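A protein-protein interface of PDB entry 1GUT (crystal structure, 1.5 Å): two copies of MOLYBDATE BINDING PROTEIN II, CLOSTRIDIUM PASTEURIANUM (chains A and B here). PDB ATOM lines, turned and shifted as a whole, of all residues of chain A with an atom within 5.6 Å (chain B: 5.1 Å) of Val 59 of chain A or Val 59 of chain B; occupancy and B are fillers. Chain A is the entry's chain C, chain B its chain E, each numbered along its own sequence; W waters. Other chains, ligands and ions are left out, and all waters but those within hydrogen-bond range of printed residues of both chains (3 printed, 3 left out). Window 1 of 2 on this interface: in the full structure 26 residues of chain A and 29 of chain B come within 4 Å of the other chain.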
ATOM      1  N   ASN A   7       4.649  -6.905 -28.099  1.00  0.00           N
ATOM      2  CA  ASN A   7       6.042  -6.497 -27.996  1.00  0.00           C
ATOM      3  C   ASN A   7       6.928  -7.487 -28.701  1.00  0.00           C
ATOM      4  O   ASN A   7       7.142  -8.581 -28.181  1.00  0.00           O
ATOM      5  CB  ASN A   7       6.442  -6.431 -26.515  1.00  0.00           C
ATOM      6  CG  ASN A   7       5.710  -5.341 -25.772  1.00  0.00           C
ATOM      7  OD1 ASN A   7       5.409  -4.292 -26.333  1.00  0.00           O
ATOM      8  ND2 ASN A   7       5.456  -5.568 -24.497  1.00  0.00           N
ATOM      9  N   GLN A   8       7.423  -7.094 -29.868  1.00  0.00           N
ATOM     10  CA  GLN A   8       8.295  -7.926 -30.695  1.00  0.00           C
ATOM     11  C   GLN A   8       9.395  -7.020 -31.188  1.00  0.00           C
ATOM     12  O   GLN A   8       9.132  -6.028 -31.894  1.00  0.00           O
ATOM     13  CB  GLN A   8       7.535  -8.478 -31.903  1.00  0.00           C
ATOM     14  CG  GLN A   8       6.382  -9.399 -31.494  1.00  0.00           C
ATOM     15  CD  GLN A   8       5.779 -10.133 -32.689  1.00  0.00           C
ATOM     16  OE1 GLN A   8       6.507 -10.630 -33.559  1.00  0.00           O
ATOM     17  NE2 GLN A   8       4.458 -10.212 -32.723  1.00  0.00           N
ATOM     18  N   ALA A  57      12.896 -10.756 -29.957  1.00  0.00           N
ATOM     19  CA  ALA A  57      12.648 -10.759 -28.512  1.00  0.00           C
ATOM     20  C   ALA A  57      11.161 -10.457 -28.295  1.00  0.00           C
ATOM     21  O   ALA A  57      10.588  -9.539 -28.930  1.00  0.00           O
ATOM     22  CB  ALA A  57      13.480  -9.668 -27.845  1.00  0.00           C
ATOM     23  N   VAL A  58      10.544 -11.166 -27.351  1.00  0.00           N
ATOM     24  CA  VAL A  58       9.119 -10.969 -27.072  1.00  0.00           C
ATOM     25  C   VAL A  58       8.942 -10.796 -25.566  1.00  0.00           C
ATOM     26  O   VAL A  58       9.512 -11.568 -24.767  1.00  0.00           O
ATOM     27  CB  VAL A  58       8.296 -12.185 -27.576  1.00  0.00           C
ATOM     28  CG1 VAL A  58       6.806 -12.004 -27.265  1.00  0.00           C
ATOM     29  CG2 VAL A  58       8.489 -12.402 -29.069  1.00  0.00           C
ATOM     30  N   VAL A  59       8.119  -9.828 -25.161  1.00  0.00           N
ATOM     31  CA  VAL A  59       7.925  -9.552 -23.724  1.00  0.00           C
ATOM     32  C   VAL A  59       6.465  -9.289 -23.413  1.00  0.00           C
ATOM     33  O   VAL A  59       5.820  -8.485 -24.087  1.00  0.00           O
ATOM     34  CB  VAL A  59       8.732  -8.296 -23.285  1.00  0.00           C
ATOM     35  CG1 VAL A  59       8.582  -8.056 -21.788  1.00  0.00           C
ATOM     36  CG2 VAL A  59      10.210  -8.401 -23.693  1.00  0.00           C
ATOM     37  N   LYS A  60       5.933  -9.961 -22.405  1.00  0.00           N
ATOM     38  CA  LYS A  60       4.543  -9.705 -22.003  1.00  0.00           C
ATOM     39  C   LYS A  60       4.466  -8.282 -21.421  1.00  0.00           C
ATOM     40  O   LYS A  60       5.313  -7.896 -20.611  1.00  0.00           O
ATOM     41  CB  LYS A  60       4.077 -10.749 -20.979  1.00  0.00           C
ATOM     42  CG  LYS A  60       2.553 -10.706 -20.704  1.00  0.00           C
ATOM     43  CD  LYS A  60       2.149 -11.825 -19.751  1.00  0.00           C
ATOM     44  CE  LYS A  60       0.625 -11.922 -19.599  1.00  0.00           C
ATOM     45  NZ  LYS A  60       0.052 -10.733 -18.903  1.00  0.00           N
ATOM     46  N   SER A  61       3.418  -7.528 -21.753  1.00  0.00           N
ATOM     47  CA  SER A  61       3.372  -6.130 -21.284  1.00  0.00           C
ATOM     48  C   SER A  61       3.369  -5.934 -19.785  1.00  0.00           C
ATOM     49  O   SER A  61       3.915  -4.952 -19.303  1.00  0.00           O
ATOM     50  CB  SER A  61       2.214  -5.374 -21.930  1.00  0.00           C
ATOM     51  OG  SER A  61       0.990  -5.923 -21.508  1.00  0.00           O
ATOM     52  N   ASP A  63       5.176  -7.355 -17.767  1.00  0.00           N
ATOM     53  CA  ASP A  63       6.544  -7.509 -17.233  1.00  0.00           C
ATOM     54  C   ASP A  63       7.395  -6.265 -17.491  1.00  0.00           C
ATOM     55  O   ASP A  63       8.591  -6.237 -17.169  1.00  0.00           O
ATOM     56  CB  ASP A  63       7.266  -8.697 -17.863  1.00  0.00           C
ATOM     57  CG  ASP A  63       6.736 -10.023 -17.387  1.00  0.00           C
ATOM     58  OD1 ASP A  63       6.253 -10.104 -16.228  1.00  0.00           O
ATOM     59  OD2 ASP A  63       6.783 -11.055 -18.118  1.00  0.00           O
ATOM     60  N   VAL A  64       6.838  -5.256 -18.145  1.00  0.00           N
ATOM     61  CA  VAL A  64       7.618  -4.048 -18.447  1.00  0.00           C
ATOM     62  C   VAL A  64       7.455  -2.961 -17.386  1.00  0.00           C
ATOM     63  O   VAL A  64       6.382  -2.389 -17.252  1.00  0.00           O
ATOM     64  CB  VAL A  64       7.230  -3.483 -19.816  1.00  0.00           C
ATOM     65  CG1 VAL A  64       8.102  -2.284 -20.155  1.00  0.00           C
ATOM     66  CG2 VAL A  64       7.337  -4.578 -20.909  1.00  0.00           C
ATOM     67  N   MET A  65       8.482  -2.747 -16.571  1.00  0.00           N
ATOM     68  CA  MET A  65       8.426  -1.671 -15.584  1.00  0.00           C
ATOM     69  C   MET A  65       8.737  -0.350 -16.281  1.00  0.00           C
ATOM     70  O   MET A  65       9.404  -0.314 -17.316  1.00  0.00           O
ATOM     71  CB  MET A  65       9.432  -1.881 -14.480  1.00  0.00           C
ATOM     72  CG  MET A  65       9.080  -3.018 -13.607  1.00  0.00           C
ATOM     73  SD  MET A  65      10.212  -3.092 -12.266  1.00  0.00           S
ATOM     74  CE  MET A  65       9.659  -1.725 -11.296  1.00  0.00           C
ATOM     75  N   ALA B   5      18.323  -5.055 -13.674  1.00  0.00           N
ATOM     76  CA  ALA B   5      17.602  -5.402 -14.919  1.00  0.00           C
ATOM     77  C   ALA B   5      18.455  -4.997 -16.114  1.00  0.00           C
ATOM     78  O   ALA B   5      18.809  -3.845 -16.277  1.00  0.00           O
ATOM     79  CB  ALA B   5      16.220  -4.724 -14.962  1.00  0.00           C
ATOM     80  N   ARG B   6      18.776  -5.966 -16.963  1.00  0.00           N
ATOM     81  CA  ARG B   6      19.683  -5.701 -18.084  1.00  0.00           C
ATOM     82  C   ARG B   6      19.093  -4.960 -19.270  1.00  0.00           C
ATOM     83  O   ARG B   6      19.836  -4.460 -20.100  1.00  0.00           O
ATOM     84  CB  ARG B   6      20.334  -7.004 -18.553  1.00  0.00           C
ATOM     85  CG  ARG B   6      21.130  -7.730 -17.474  1.00  0.00           C
ATOM     86  CD  ARG B   6      22.418  -7.084 -17.174  1.00  0.00           C
ATOM     87  NE  ARG B   6      23.349  -7.064 -18.303  1.00  0.00           N
ATOM     88  CZ  ARG B   6      24.542  -6.514 -18.196  1.00  0.00           C
ATOM     89  NH1 ARG B   6      24.893  -5.979 -17.032  1.00  0.00           N
ATOM     90  NH2 ARG B   6      25.384  -6.497 -19.218  1.00  0.00           N
ATOM     91  N   ASN B   7      17.767  -4.886 -19.346  1.00  0.00           N
ATOM     92  CA  ASN B   7      17.096  -4.202 -20.440  1.00  0.00           C
ATOM     93  C   ASN B   7      16.533  -2.888 -19.935  1.00  0.00           C
ATOM     94  O   ASN B   7      15.612  -2.881 -19.105  1.00  0.00           O
ATOM     95  CB  ASN B   7      16.006  -5.100 -20.974  1.00  0.00           C
ATOM     96  CG  ASN B   7      16.569  -6.391 -21.435  1.00  0.00           C
ATOM     97  OD1 ASN B   7      17.329  -6.404 -22.402  1.00  0.00           O
ATOM     98  ND2 ASN B   7      16.284  -7.483 -20.712  1.00  0.00           N
ATOM     99  N   ILE B  35       7.256  -0.355 -27.387  1.00  0.00           N
ATOM    100  CA  ILE B  35       7.104  -1.331 -26.322  1.00  0.00           C
ATOM    101  C   ILE B  35       5.934  -0.907 -25.443  1.00  0.00           C
ATOM    102  O   ILE B  35       5.830   0.243 -25.047  1.00  0.00           O
ATOM    103  CB  ILE B  35       8.426  -1.594 -25.558  1.00  0.00           C
ATOM    104  CG1 ILE B  35       8.262  -2.796 -24.617  1.00  0.00           C
ATOM    105  CG2 ILE B  35       8.889  -0.357 -24.819  1.00  0.00           C
ATOM    106  CD1 ILE B  35       9.572  -3.255 -23.951  1.00  0.00           C
ATOM    107  N   ALA B  57      11.824   1.945 -20.245  1.00  0.00           N
ATOM    108  CA  ALA B  57      11.179   0.641 -20.089  1.00  0.00           C
ATOM    109  C   ALA B  57      12.248  -0.291 -19.510  1.00  0.00           C
ATOM    110  O   ALA B  57      13.352  -0.416 -20.063  1.00  0.00           O
ATOM    111  CB  ALA B  57      10.684   0.117 -21.416  1.00  0.00           C
ATOM    112  N   VAL B  58      11.923  -0.968 -18.416  1.00  0.00           N
ATOM    113  CA  VAL B  58      12.888  -1.815 -17.716  1.00  0.00           C
ATOM    114  C   VAL B  58      12.352  -3.236 -17.632  1.00  0.00           C
ATOM    115  O   VAL B  58      11.279  -3.492 -17.065  1.00  0.00           O
ATOM    116  CB  VAL B  58      13.150  -1.228 -16.312  1.00  0.00           C
ATOM    117  CG1 VAL B  58      14.127  -2.064 -15.530  1.00  0.00           C
ATOM    118  CG2 VAL B  58      13.691   0.209 -16.423  1.00  0.00           C
ATOM    119  N   VAL B  59      13.105  -4.159 -18.218  1.00  0.00           N
ATOM    120  CA  VAL B  59      12.717  -5.555 -18.316  1.00  0.00           C
ATOM    121  C   VAL B  59      13.790  -6.515 -17.850  1.00  0.00           C
ATOM    122  O   VAL B  59      14.951  -6.390 -18.238  1.00  0.00           O
ATOM    123  CB  VAL B  59      12.369  -5.899 -19.789  1.00  0.00           C
ATOM    124  CG1 VAL B  59      11.825  -7.308 -19.891  1.00  0.00           C
ATOM    125  CG2 VAL B  59      11.329  -4.917 -20.316  1.00  0.00           C
ATOM    126  N   LYS B  60      13.412  -7.417 -16.939  1.00  0.00           N
ATOM    127  CA  LYS B  60      14.334  -8.453 -16.466  1.00  0.00           C
ATOM    128  C   LYS B  60      14.609  -9.442 -17.612  1.00  0.00           C
ATOM    129  O   LYS B  60      13.699  -9.797 -18.385  1.00  0.00           O
ATOM    130  CB  LYS B  60      13.704  -9.201 -15.290  1.00  0.00           C
ATOM    131  CG  LYS B  60      13.482  -8.282 -14.076  1.00  0.00           C
ATOM    132  CD  LYS B  60      12.632  -8.956 -13.001  1.00  0.00           C
ATOM    133  CE  LYS B  60      11.154  -9.040 -13.325  1.00  0.00           C
ATOM    134  NZ  LYS B  60      10.511  -7.706 -13.347  1.00  0.00           N
ATOM    135  N   SER B  61      15.862  -9.885 -17.728  1.00  0.00           N
ATOM    136  CA  SER B  61      16.247 -10.828 -18.780  1.00  0.00           C
ATOM    137  C   SER B  61      15.417 -12.103 -18.785  1.00  0.00           C
ATOM    138  O   SER B  61      15.146 -12.639 -19.847  1.00  0.00           O
ATOM    139  CB  SER B  61      17.738 -11.193 -18.659  1.00  0.00           C
ATOM    140  OG  SER B  61      18.518 -10.035 -18.765  1.00  0.00           O
ATOM    141  N   ASP B  63      12.424 -12.384 -18.342  1.00  0.00           N
ATOM    142  CA  ASP B  63      11.087 -12.126 -18.881  1.00  0.00           C
ATOM    143  C   ASP B  63      11.130 -11.954 -20.383  1.00  0.00           C
ATOM    144  O   ASP B  63      10.109 -11.696 -20.999  1.00  0.00           O
ATOM    145  CB  ASP B  63      10.444 -10.891 -18.243  1.00  0.00           C
ATOM    146  CG  ASP B  63       9.955 -11.171 -16.869  1.00  0.00           C
ATOM    147  OD1 ASP B  63       9.730 -12.368 -16.535  1.00  0.00           O
ATOM    148  OD2 ASP B  63       9.729 -10.251 -16.071  1.00  0.00           O
ATOM    149  N   VAL B  64      12.308 -12.075 -20.983  1.00  0.00           N
ATOM    150  CA  VAL B  64      12.401 -11.916 -22.440  1.00  0.00           C
ATOM    151  C   VAL B  64      12.390 -13.279 -23.120  1.00  0.00           C
ATOM    152  O   VAL B  64      13.269 -14.111 -22.841  1.00  0.00           O
ATOM    153  CB  VAL B  64      13.682 -11.152 -22.866  1.00  0.00           C
ATOM    154  CG1 VAL B  64      13.737 -11.009 -24.405  1.00  0.00           C
ATOM    155  CG2 VAL B  64      13.742  -9.772 -22.205  1.00  0.00           C
ATOM    156  N   MET B  65      11.375 -13.527 -23.959  1.00  0.00           N
ATOM    157  CA  MET B  65      11.309 -14.773 -24.715  1.00  0.00           C
ATOM    158  C   MET B  65      11.955 -14.553 -26.062  1.00  0.00           C
ATOM    159  O   MET B  65      12.051 -13.420 -26.528  1.00  0.00           O
ATOM    160  CB  MET B  65       9.844 -15.155 -24.911  1.00  0.00           C
ATOM    161  CG  MET B  65       9.188 -15.547 -23.621  1.00  0.00           C
ATOM    162  SD  MET B  65       7.404 -15.594 -23.740  1.00  0.00           S
ATOM    163  CE  MET B  65       7.009 -13.816 -23.807  1.00  0.00           C
HETATM  164  O   HOH W   1       7.458 -11.635 -20.613  1.00  0.00           O
HETATM  165  O   HOH W   2      11.514  -5.188 -14.549  1.00  0.00           O
HETATM  166  O   HOH W   3      10.637  -7.671 -16.263  1.00  0.00           O
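ND2 of Asn 7 of chain A is in hydrogen-bond range of O of Val 59 of chain A (3.0 Å). The backbone NH (N) of Val 59 of chain B lies within hydrogen-bond range of the backbone carbonyl oxygen (O) of Asn 7 of chain B, at 3.0 Å. The side-chain carboxylate (OD2) of Asp 63 of chain B lies within salt-bridge range of the side-chain amino group (NZ) of Lys 60 of chain B (3.8 Å).
Among the printed residues, pairs that only touch across the chains: Ala 57 of chain A with Met 65 of chain B, Asn 7 of chain A with Ile 35 of chain B, Met 65 of chain A with Ala 57 of chain B, Ala 57 of chain A with Val 64 of chain B, Val 58 of chain A with Val 64 of chain B, Val 64 of chain A with Ala 57 of chain B, Val 58 of chain A with Asp 63 of chain B, Val 59 of chain A with Val 59 of chain B, Asp 63 of chain A with Val 58 of chain B, Val 64 of chain A with Val 58 of chain B and Val 64 of chain A with Ile 35 of chain B.
Printed residues of chain A that touch a printed residue of chain B: Asn 7, Ala 57, Val 58, Val 59, Asp 63, Val 64 and Met 65. Hydrophobic or aromatic side chains of chain A that line the printed part of chain B: Ala 57, Val 58, Val 59, Val 64 and Met 65. Among the printed residues, no Asp or Glu carboxylate lies within 4 Å of a Lys or Arg side-chain nitrogen of the other chain.
Water W1 lies within hydrogen-bond range of the side-chain carboxylate of Asp 63 of chain A (2.6 Å), the backbone carbonyl oxygen of Asp 63 of chain B (2.7 Å) and the backbone NH of Lys 60 of chain A (2.9 Å). Water W3 lies within hydrogen-bond range of the backbone carbonyl oxygen of Asp 63 of chain A, the side-chain carboxylate of Asp 63 of chain B and the backbone NH of Lys 60 of chain B. Water W2 lies within hydrogen-bond range of the side-chain amino group of Lys 60 of chain B (3.0 Å), the backbone carbonyl oxygen of Val 58 of chain B (3.0 Å) and the side-chain sulfur of Met 65 of chain A (3.4 Å).
Val 59 of chain A touches just one residue of chain B: Val 59. Val 59 of chain B touches just one residue of chain A: Val 59 (3.8 Å). Printed residues of chain A within 4 Å of Met 65 of chain B: Ala 57 and Val 58. Of the printed residues of chain A, Asp 63 of chain B touches Val 58 and Asp 63. Of the printed residues of chain B, Asn 7 of chain A touches Ile 35 (3.4 Å). Asn 7 of chain B touches none of the printed residues of chain A. Ser 61 of chain A touches none of the printed residues of chain B. The nearest residue of chain A that does not touch Val 59 of chain B is Val 64 of chain A (4.1 Å). The nearest printed residue of chain B that does not touch Asn 7 of chain A is Met 65 of chain B (6.8 Å).
The backbone carbonyl oxygen of Val 58 of chain A sits at hydrogen-bond distance from the backbone NH of Met 65 of chain B, at 2.8 Å. The backbone carbonyl oxygen (O) of Met 65 of chain A sits at hydrogen-bond distance from the backbone NH (N) of Val 58 of chain B (2.8 Å). The side-chain carboxylate (OD2) of Asp 63 of chain B lies close to the side-chain carboxylate (OD1) of Asp 63 of chain A.
Ala 57 of chain A touches Val 64 of chain B, and with the chains exchanged Val 64 of chain A touches Ala 57 of chain B. Ala 57 of chain A touches Met 65 of chain B, and with the chains exchanged Met 65 of chain A touches Ala 57 of chain B. Val 58 of chain A touches Asp 63 of chain B, and with the chains exchanged Asp 63 of chain A touches Val 58 of chain B. Val 59 of chain B touches its own counterpart, Val 59 of chain A.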
